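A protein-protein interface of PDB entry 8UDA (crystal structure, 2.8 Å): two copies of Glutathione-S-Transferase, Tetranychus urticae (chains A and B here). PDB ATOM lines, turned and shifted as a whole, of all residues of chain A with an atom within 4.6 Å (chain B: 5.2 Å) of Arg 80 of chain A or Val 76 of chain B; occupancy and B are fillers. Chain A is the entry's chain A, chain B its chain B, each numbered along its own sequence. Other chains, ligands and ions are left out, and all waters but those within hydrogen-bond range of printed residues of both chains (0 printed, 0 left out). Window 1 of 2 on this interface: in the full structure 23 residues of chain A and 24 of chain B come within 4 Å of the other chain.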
ATOM      1  N   VAL A  76      25.585   0.806   8.481  1.00  0.00           N
ATOM      2  CA  VAL A  76      25.863  -0.114   7.380  1.00  0.00           C
ATOM      3  C   VAL A  76      27.377  -0.280   7.210  1.00  0.00           C
ATOM      4  O   VAL A  76      27.882  -1.398   7.037  1.00  0.00           O
ATOM      5  CB  VAL A  76      25.231   0.289   6.024  1.00  0.00           C
ATOM      6  CG1 VAL A  76      25.569  -0.765   4.982  1.00  0.00           C
ATOM      7  CG2 VAL A  76      23.718   0.517   6.036  1.00  0.00           C
ATOM      8  N   ALA A  77      28.096   0.853   7.239  1.00  0.00           N
ATOM      9  CA  ALA A  77      29.545   0.852   7.128  1.00  0.00           C
ATOM     10  C   ALA A  77      30.151  -0.049   8.205  1.00  0.00           C
ATOM     11  O   ALA A  77      30.958  -0.948   7.894  1.00  0.00           O
ATOM     12  CB  ALA A  77      30.068   2.272   7.186  1.00  0.00           C
ATOM     13  N   ILE A  78      29.724   0.179   9.465  1.00  0.00           N
ATOM     14  CA  ILE A  78      30.167  -0.621  10.603  1.00  0.00           C
ATOM     15  C   ILE A  78      29.873  -2.109  10.358  1.00  0.00           C
ATOM     16  O   ILE A  78      30.748  -2.952  10.560  1.00  0.00           O
ATOM     17  CB  ILE A  78      29.525  -0.163  11.927  1.00  0.00           C
ATOM     18  CG1 ILE A  78      29.878   1.278  12.300  1.00  0.00           C
ATOM     19  CG2 ILE A  78      29.890  -1.132  13.042  1.00  0.00           C
ATOM     20  CD1 ILE A  78      28.869   1.912  13.251  1.00  0.00           C
ATOM     21  N   ILE A  79      28.642  -2.448   9.940  1.00  0.00           N
ATOM     22  CA  ILE A  79      28.327  -3.860   9.837  1.00  0.00           C
ATOM     23  C   ILE A  79      29.075  -4.469   8.653  1.00  0.00           C
ATOM     24  O   ILE A  79      29.505  -5.613   8.734  1.00  0.00           O
ATOM     25  CB  ILE A  79      26.809  -4.124   9.822  1.00  0.00           C
ATOM     26  CG1 ILE A  79      26.495  -5.558  10.275  1.00  0.00           C
ATOM     27  CG2 ILE A  79      26.209  -3.756   8.474  1.00  0.00           C
ATOM     28  CD1 ILE A  79      25.027  -5.891  10.395  1.00  0.00           C
ATOM     29  N   ARG A  80      29.257  -3.717   7.560  1.00  0.00           N
ATOM     30  CA  ARG A  80      29.996  -4.244   6.425  1.00  0.00           C
ATOM     31  C   ARG A  80      31.467  -4.453   6.809  1.00  0.00           C
ATOM     32  O   ARG A  80      32.097  -5.435   6.394  1.00  0.00           O
ATOM     33  CB  ARG A  80      29.869  -3.344   5.192  1.00  0.00           C
ATOM     34  CG  ARG A  80      28.536  -3.346   4.458  1.00  0.00           C
ATOM     35  CD  ARG A  80      28.826  -2.611   3.153  1.00  0.00           C
ATOM     36  NE  ARG A  80      27.661  -2.332   2.326  1.00  0.00           N
ATOM     37  CZ  ARG A  80      27.242  -1.113   1.949  1.00  0.00           C
ATOM     38  NH1 ARG A  80      27.823  -0.037   2.453  1.00  0.00           N
ATOM     39  NH2 ARG A  80      26.245  -0.960   1.079  1.00  0.00           N
ATOM     40  N   TYR A  81      32.032  -3.525   7.595  1.00  0.00           N
ATOM     41  CA  TYR A  81      33.394  -3.706   8.084  1.00  0.00           C
ATOM     42  C   TYR A  81      33.542  -5.044   8.827  1.00  0.00           C
ATOM     43  O   TYR A  81      34.459  -5.818   8.539  1.00  0.00           O
ATOM     44  CB  TYR A  81      33.780  -2.569   9.029  1.00  0.00           C
ATOM     45  CG  TYR A  81      34.981  -2.877   9.886  1.00  0.00           C
ATOM     46  CD1 TYR A  81      36.240  -3.029   9.318  1.00  0.00           C
ATOM     47  CD2 TYR A  81      34.868  -3.046  11.264  1.00  0.00           C
ATOM     48  CE1 TYR A  81      37.353  -3.313  10.098  1.00  0.00           C
ATOM     49  CE2 TYR A  81      35.978  -3.330  12.051  1.00  0.00           C
ATOM     50  CZ  TYR A  81      37.228  -3.463  11.470  1.00  0.00           C
ATOM     51  OH  TYR A  81      38.342  -3.731  12.232  1.00  0.00           O
ATOM     52  N   LEU A  82      32.643  -5.294   9.794  1.00  0.00           N
ATOM     53  CA  LEU A  82      32.646  -6.479  10.636  1.00  0.00           C
ATOM     54  C   LEU A  82      32.355  -7.727   9.803  1.00  0.00           C
ATOM     55  O   LEU A  82      32.953  -8.787  10.014  1.00  0.00           O
ATOM     56  CB  LEU A  82      31.583  -6.316  11.722  1.00  0.00           C
ATOM     57  CG  LEU A  82      31.842  -5.229  12.769  1.00  0.00           C
ATOM     58  CD1 LEU A  82      30.732  -5.214  13.816  1.00  0.00           C
ATOM     59  CD2 LEU A  82      33.216  -5.398  13.447  1.00  0.00           C
ATOM     60  N   ALA A  83      31.414  -7.600   8.864  1.00  0.00           N
ATOM     61  CA  ALA A  83      31.119  -8.683   7.944  1.00  0.00           C
ATOM     62  C   ALA A  83      32.394  -9.098   7.217  1.00  0.00           C
ATOM     63  O   ALA A  83      32.668 -10.291   7.122  1.00  0.00           O
ATOM     64  CB  ALA A  83      30.032  -8.270   6.997  1.00  0.00           C
ATOM     65  N   ARG A  84      33.181  -8.115   6.745  1.00  0.00           N
ATOM     66  CA  ARG A  84      34.414  -8.401   6.019  1.00  0.00           C
ATOM     67  C   ARG A  84      35.412  -9.129   6.933  1.00  0.00           C
ATOM     68  O   ARG A  84      35.987 -10.142   6.528  1.00  0.00           O
ATOM     69  CB  ARG A  84      35.024  -7.138   5.409  1.00  0.00           C
ATOM     70  CG  ARG A  84      34.335  -6.667   4.135  1.00  0.00           C
ATOM     71  CD  ARG A  84      34.879  -5.365   3.602  1.00  0.00           C
ATOM     72  NE  ARG A  84      34.817  -4.257   4.558  1.00  0.00           N
ATOM     73  CZ  ARG A  84      34.020  -3.193   4.487  1.00  0.00           C
ATOM     74  NH1 ARG A  84      34.332  -2.103   5.177  1.00  0.00           N
ATOM     75  NH2 ARG A  84      32.957  -3.196   3.690  1.00  0.00           N
ATOM     76  N   GLU A 103      20.224  -6.190   1.666  1.00  0.00           N
ATOM     77  CA  GLU A 103      20.664  -5.171   2.602  1.00  0.00           C
ATOM     78  C   GLU A 103      19.824  -3.911   2.432  1.00  0.00           C
ATOM     79  O   GLU A 103      19.298  -3.362   3.385  1.00  0.00           O
ATOM     80  CB  GLU A 103      22.125  -4.831   2.332  1.00  0.00           C
ATOM     81  CG  GLU A 103      22.637  -3.671   3.170  1.00  0.00           C
ATOM     82  CD  GLU A 103      23.955  -3.158   2.616  1.00  0.00           C
ATOM     83  OE1 GLU A 103      23.950  -2.044   2.022  1.00  0.00           O
ATOM     84  OE2 GLU A 103      24.965  -3.914   2.706  1.00  0.00           O
ATOM     85  N   GLN A 104      19.690  -3.459   1.188  1.00  0.00           N
ATOM     86  CA  GLN A 104      19.002  -2.214   0.890  1.00  0.00           C
ATOM     87  C   GLN A 104      17.511  -2.362   1.130  1.00  0.00           C
ATOM     88  O   GLN A 104      16.883  -1.427   1.606  1.00  0.00           O
ATOM     89  CB  GLN A 104      19.325  -1.759  -0.530  1.00  0.00           C
ATOM     90  CG  GLN A 104      20.794  -1.403  -0.675  1.00  0.00           C
ATOM     91  CD  GLN A 104      21.059  -0.201   0.187  1.00  0.00           C
ATOM     92  OE1 GLN A 104      20.321   0.782   0.135  1.00  0.00           O
ATOM     93  NE2 GLN A 104      22.107  -0.281   0.990  1.00  0.00           N
ATOM     94  N   TYR A 160      25.787 -11.183   6.859  1.00  0.00           N
ATOM     95  CA  TYR A 160      25.469 -10.124   7.809  1.00  0.00           C
ATOM     96  C   TYR A 160      24.020  -9.667   7.619  1.00  0.00           C
ATOM     97  O   TYR A 160      23.407  -9.110   8.520  1.00  0.00           O
ATOM     98  CB  TYR A 160      26.478  -8.977   7.654  1.00  0.00           C
ATOM     99  CG  TYR A 160      26.405  -8.175   6.376  1.00  0.00           C
ATOM    100  CD1 TYR A 160      25.490  -7.131   6.209  1.00  0.00           C
ATOM    101  CD2 TYR A 160      27.257  -8.458   5.319  1.00  0.00           C
ATOM    102  CE1 TYR A 160      25.455  -6.388   5.030  1.00  0.00           C
ATOM    103  CE2 TYR A 160      27.216  -7.737   4.133  1.00  0.00           C
ATOM    104  CZ  TYR A 160      26.333  -6.684   3.995  1.00  0.00           C
ATOM    105  OH  TYR A 160      26.297  -6.013   2.795  1.00  0.00           O
ATOM    106  N   GLN B  74      18.295  -2.309  -6.498  1.00  0.00           N
ATOM    107  CA  GLN B  74      18.541  -1.341  -5.416  1.00  0.00           C
ATOM    108  C   GLN B  74      19.624  -0.327  -5.805  1.00  0.00           C
ATOM    109  O   GLN B  74      20.719  -0.722  -6.160  1.00  0.00           O
ATOM    110  CB  GLN B  74      18.876  -2.022  -4.085  1.00  0.00           C
ATOM    111  CG  GLN B  74      17.848  -3.061  -3.641  1.00  0.00           C
ATOM    112  CD  GLN B  74      16.537  -2.403  -3.295  1.00  0.00           C
ATOM    113  OE1 GLN B  74      16.493  -1.506  -2.459  1.00  0.00           O
ATOM    114  NE2 GLN B  74      15.477  -2.800  -3.987  1.00  0.00           N
ATOM    115  N   THR B  75      19.332   0.975  -5.725  1.00  0.00           N
ATOM    116  CA  THR B  75      20.224   2.021  -6.206  1.00  0.00           C
ATOM    117  C   THR B  75      21.652   1.797  -5.707  1.00  0.00           C
ATOM    118  O   THR B  75      22.566   1.721  -6.541  1.00  0.00           O
ATOM    119  CB  THR B  75      19.735   3.408  -5.775  1.00  0.00           C
ATOM    120  OG1 THR B  75      18.365   3.565  -6.145  1.00  0.00           O
ATOM    121  CG2 THR B  75      20.591   4.543  -6.291  1.00  0.00           C
ATOM    122  N   VAL B  76      21.827   1.646  -4.368  1.00  0.00           N
ATOM    123  CA  VAL B  76      23.159   1.442  -3.800  1.00  0.00           C
ATOM    124  C   VAL B  76      23.751   0.151  -4.365  1.00  0.00           C
ATOM    125  O   VAL B  76      24.890   0.157  -4.840  1.00  0.00           O
ATOM    126  CB  VAL B  76      23.202   1.460  -2.254  1.00  0.00           C
ATOM    127  CG1 VAL B  76      24.565   1.026  -1.738  1.00  0.00           C
ATOM    128  CG2 VAL B  76      22.862   2.822  -1.660  1.00  0.00           C
ATOM    129  N   ALA B  77      22.955  -0.935  -4.329  1.00  0.00           N
ATOM    130  CA  ALA B  77      23.394  -2.230  -4.836  1.00  0.00           C
ATOM    131  C   ALA B  77      23.874  -2.101  -6.280  1.00  0.00           C
ATOM    132  O   ALA B  77      25.001  -2.505  -6.599  1.00  0.00           O
ATOM    133  CB  ALA B  77      22.321  -3.273  -4.662  1.00  0.00           C
ATOM    134  N   ILE B  78      23.046  -1.448  -7.109  1.00  0.00           N
ATOM    135  CA  ILE B  78      23.383  -1.166  -8.506  1.00  0.00           C
ATOM    136  C   ILE B  78      24.710  -0.409  -8.628  1.00  0.00           C
ATOM    137  O   ILE B  78      25.581  -0.807  -9.405  1.00  0.00           O
ATOM    138  CB  ILE B  78      22.254  -0.437  -9.261  1.00  0.00           C
ATOM    139  CG1 ILE B  78      20.961  -1.253  -9.287  1.00  0.00           C
ATOM    140  CG2 ILE B  78      22.715  -0.086 -10.664  1.00  0.00           C
ATOM    141  CD1 ILE B  78      19.741  -0.400  -9.481  1.00  0.00           C
ATOM    142  N   ILE B  79      24.852   0.684  -7.876  1.00  0.00           N
ATOM    143  CA  ILE B  79      26.050   1.493  -8.016  1.00  0.00           C
ATOM    144  C   ILE B  79      27.272   0.726  -7.503  1.00  0.00           C
ATOM    145  O   ILE B  79      28.338   0.826  -8.103  1.00  0.00           O
ATOM    146  CB  ILE B  79      25.889   2.888  -7.379  1.00  0.00           C
ATOM    147  CG1 ILE B  79      26.878   3.894  -7.966  1.00  0.00           C
ATOM    148  CG2 ILE B  79      25.971   2.819  -5.861  1.00  0.00           C
ATOM    149  CD1 ILE B  79      26.591   5.328  -7.596  1.00  0.00           C
ATOM    150  N   ARG B  80      27.120  -0.054  -6.421  1.00  0.00           N
ATOM    151  CA  ARG B  80      28.255  -0.797  -5.892  1.00  0.00           C
ATOM    152  C   ARG B  80      28.647  -1.891  -6.885  1.00  0.00           C
ATOM    153  O   ARG B  80      29.826  -2.136  -7.096  1.00  0.00           O
ATOM    154  CB  ARG B  80      27.972  -1.363  -4.500  1.00  0.00           C
ATOM    155  CG  ARG B  80      27.848  -0.301  -3.421  1.00  0.00           C
ATOM    156  CD  ARG B  80      27.400  -0.836  -2.070  1.00  0.00           C
ATOM    157  NE  ARG B  80      28.219  -1.868  -1.442  1.00  0.00           N
ATOM    158  CZ  ARG B  80      29.465  -1.756  -0.972  1.00  0.00           C
ATOM    159  NH1 ARG B  80      30.083  -0.587  -0.916  1.00  0.00           N
ATOM    160  NH2 ARG B  80      30.080  -2.837  -0.513  1.00  0.00           N
ATOM    161  N   TYR B  81      27.655  -2.532  -7.512  1.00  0.00           N
ATOM    162  CA  TYR B  81      27.946  -3.513  -8.546  1.00  0.00           C
ATOM    163  C   TYR B  81      28.848  -2.906  -9.640  1.00  0.00           C
ATOM    164  O   TYR B  81      29.874  -3.493  -9.999  1.00  0.00           O
ATOM    165  CB  TYR B  81      26.639  -4.033  -9.155  1.00  0.00           C
ATOM    166  CG  TYR B  81      26.853  -4.714 -10.485  1.00  0.00           C
ATOM    167  CD1 TYR B  81      27.507  -5.939 -10.533  1.00  0.00           C
ATOM    168  CD2 TYR B  81      26.452  -4.141 -11.700  1.00  0.00           C
ATOM    169  CE1 TYR B  81      27.748  -6.575 -11.743  1.00  0.00           C
ATOM    170  CE2 TYR B  81      26.714  -4.756 -12.918  1.00  0.00           C
ATOM    171  CZ  TYR B  81      27.351  -5.986 -12.939  1.00  0.00           C
ATOM    172  OH  TYR B  81      27.627  -6.639 -14.121  1.00  0.00           O
ATOM    173  N   GLU B 100      32.447   4.006   2.623  1.00  0.00           N
ATOM    174  CA  GLU B 100      31.131   3.498   2.985  1.00  0.00           C
ATOM    175  C   GLU B 100      30.496   4.408   4.038  1.00  0.00           C
ATOM    176  O   GLU B 100      29.281   4.545   4.090  1.00  0.00           O
ATOM    177  CB  GLU B 100      31.202   2.001   3.339  1.00  0.00           C
ATOM    178  CG  GLU B 100      31.523   1.088   2.145  1.00  0.00           C
ATOM    179  CD  GLU B 100      31.678  -0.400   2.453  1.00  0.00           C
ATOM    180  OE1 GLU B 100      31.822  -0.760   3.668  1.00  0.00           O
ATOM    181  OE2 GLU B 100      31.644  -1.229   1.487  1.00  0.00           O
ATOM    182  N   GLU B 103      29.192   7.078   1.824  1.00  0.00           N
ATOM    183  CA  GLU B 103      28.033   6.520   1.135  1.00  0.00           C
ATOM    184  C   GLU B 103      26.776   6.688   1.985  1.00  0.00           C
ATOM    185  O   GLU B 103      25.767   7.226   1.523  1.00  0.00           O
ATOM    186  CB  GLU B 103      28.232   5.036   0.848  1.00  0.00           C
ATOM    187  CG  GLU B 103      26.990   4.352   0.322  1.00  0.00           C
ATOM    188  CD  GLU B 103      27.115   2.839   0.313  1.00  0.00           C
ATOM    189  OE1 GLU B 103      28.084   2.329  -0.306  1.00  0.00           O
ATOM    190  OE2 GLU B 103      26.258   2.170   0.947  1.00  0.00           O
ATOM    191  N   GLN B 104      26.871   6.247   3.240  1.00  0.00           N
ATOM    192  CA  GLN B 104      25.721   6.231   4.130  1.00  0.00           C
ATOM    193  C   GLN B 104      25.347   7.665   4.497  1.00  0.00           C
ATOM    194  O   GLN B 104      24.166   7.979   4.645  1.00  0.00           O
ATOM    195  CB  GLN B 104      26.003   5.358   5.361  1.00  0.00           C
ATOM    196  CG  GLN B 104      26.319   3.908   5.015  1.00  0.00           C
ATOM    197  CD  GLN B 104      25.119   3.305   4.323  1.00  0.00           C
ATOM    198  OE1 GLN B 104      24.001   3.377   4.820  1.00  0.00           O
ATOM    199  NE2 GLN B 104      25.325   2.744   3.141  1.00  0.00           N
ATOM    200  N   ILE B 107      23.182   8.993   1.773  1.00  0.00           N
ATOM    201  CA  ILE B 107      21.855   8.397   1.892  1.00  0.00           C
ATOM    202  C   ILE B 107      21.055   9.094   3.001  1.00  0.00           C
ATOM    203  O   ILE B 107      19.860   9.358   2.826  1.00  0.00           O
ATOM    204  CB  ILE B 107      21.977   6.877   2.138  1.00  0.00           C
ATOM    205  CG1 ILE B 107      22.580   6.140   0.942  1.00  0.00           C
ATOM    206  CG2 ILE B 107      20.685   6.239   2.595  1.00  0.00           C
ATOM    207  CD1 ILE B 107      22.962   4.722   1.293  1.00  0.00           C
ATOM    208  N   MET B 164      27.450   9.805  -5.950  1.00  0.00           N
ATOM    209  CA  MET B 164      26.373   9.853  -4.978  1.00  0.00           C
ATOM    210  C   MET B 164      26.299  11.261  -4.388  1.00  0.00           C
ATOM    211  O   MET B 164      25.275  11.948  -4.473  1.00  0.00           O
ATOM    212  CB  MET B 164      26.671   8.858  -3.853  1.00  0.00           C
ATOM    213  CG  MET B 164      26.535   7.425  -4.305  1.00  0.00           C
ATOM    214  SD  MET B 164      26.576   6.255  -2.954  1.00  0.00           S
ATOM    215  CE  MET B 164      24.966   6.548  -2.212  1.00  0.00           C
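The side-chain carboxylate of Glu 103 of chain B is in salt-bridge range of the guanidinium group of Arg 80 of chain A (3.1 Å). The side-chain carboxylate (OE1) of Glu 100 of chain B is in salt-bridge range of the guanidinium group (NH2) of Arg 84 of chain A, at 2.7 Å. NH2 of Arg 80 of chain A lies close to NE of Arg 80 of chain B.
The backbone carbonyl oxygen of Arg 80 of chain A lies close to the guanidinium group of Arg 84 of chain A (3.5 Å). The guanidinium group (NH2) of Arg 80 of chain A is in salt-bridge range of the side-chain carboxylate (OE1) of Glu 103 of chain A (2.7 Å). The side-chain carboxylate of Glu 103 of chain A lies within hydrogen-bond range of the side-chain amide nitrogen of Gln 104 of chain A (2.8 Å). The guanidinium group (NH1) of Arg 80 of chain B is in salt-bridge range of the side-chain carboxylate (OE2) of Glu 100 of chain B (2.9 Å). NH1 of Arg 80 of chain B is in salt-bridge range of OE1 of Glu 103 of chain B, at 3.6 Å. The side-chain carboxylate (OE2) of Glu 103 of chain B lies within hydrogen-bond range of the side-chain amide nitrogen (NE2) of Gln 104 of chain B, 2.5 Å away.
Gln 104 of chain B touches Val 76 of chain A. CB of Ala 77 of chain A touches C of Glu 100 of chain B, at 3.8 Å. Arg 80 of chain A touches Val 76 of chain B. Glu 100 of chain B touches Arg 80 of chain A. Arg 80 of chain A touches Gln 104 of chain B (NH1 to NE2, 3.8 Å). Gln 104 of chain A touches Gln 74 of chain B (CB to OE1, 3.4 Å). CD of Gln 104 of chain A touches CB of Val 76 of chain B, 3.6 Å away.
Of chain B, only Val 76, Arg 80, Glu 100, Glu 103 and Gln 104 come within 4 Å of Arg 80 of chain A. Printed residues of chain A within 4 Å of Val 76 of chain B: Arg 80 and Gln 104. Printed residues of chain B within 4 Å of Gln 104 of chain A: Gln 74 and Val 76. Printed residues of chain A within 4 Å of Gln 104 of chain B: Val 76 (3.1 Å) and Arg 80 (3.8 Å). Printed residues of chain B within 4 Å of Ala 77 of chain A: Glu 100. Ala 77 of chain B touches none of the printed residues of chain A. The nearest printed residue of chain A that does not touch Val 76 of chain B is Glu 103 of chain A (4.9 Å).
Of the 12 printed residues of chain A, 5 touch a printed residue of chain B. Among the printed residues, 10 pairs touch across the chains. Among the printed residues, Asp or Glu carboxylates within 4 Å of a Lys or Arg side-chain nitrogen of the other chain: Arg 80 of chain A with Glu 103 of chain B (3.1 Å) and Arg 84 of chain A with Glu 100 of chain B (2.7 Å).
Val 76 of chain A touches Gln 104 of chain B, and with the chains exchanged Gln 104 of chain A touches Val 76 of chain B. Arg 80 of chain A touches Val 76 of chain B, but with the chains exchanged Val 76 of chain A does not touch Arg 80 of chain B (7.0 Å). Arg 80 of chain B touches its own counterpart, Arg 80 of chain A. Arg 80 of chain A touches Glu 103 of chain B, but with the chains exchanged Glu 103 of chain A does not touch Arg 80 of chain B (5.5 Å). 8 positions are printed for both chains.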
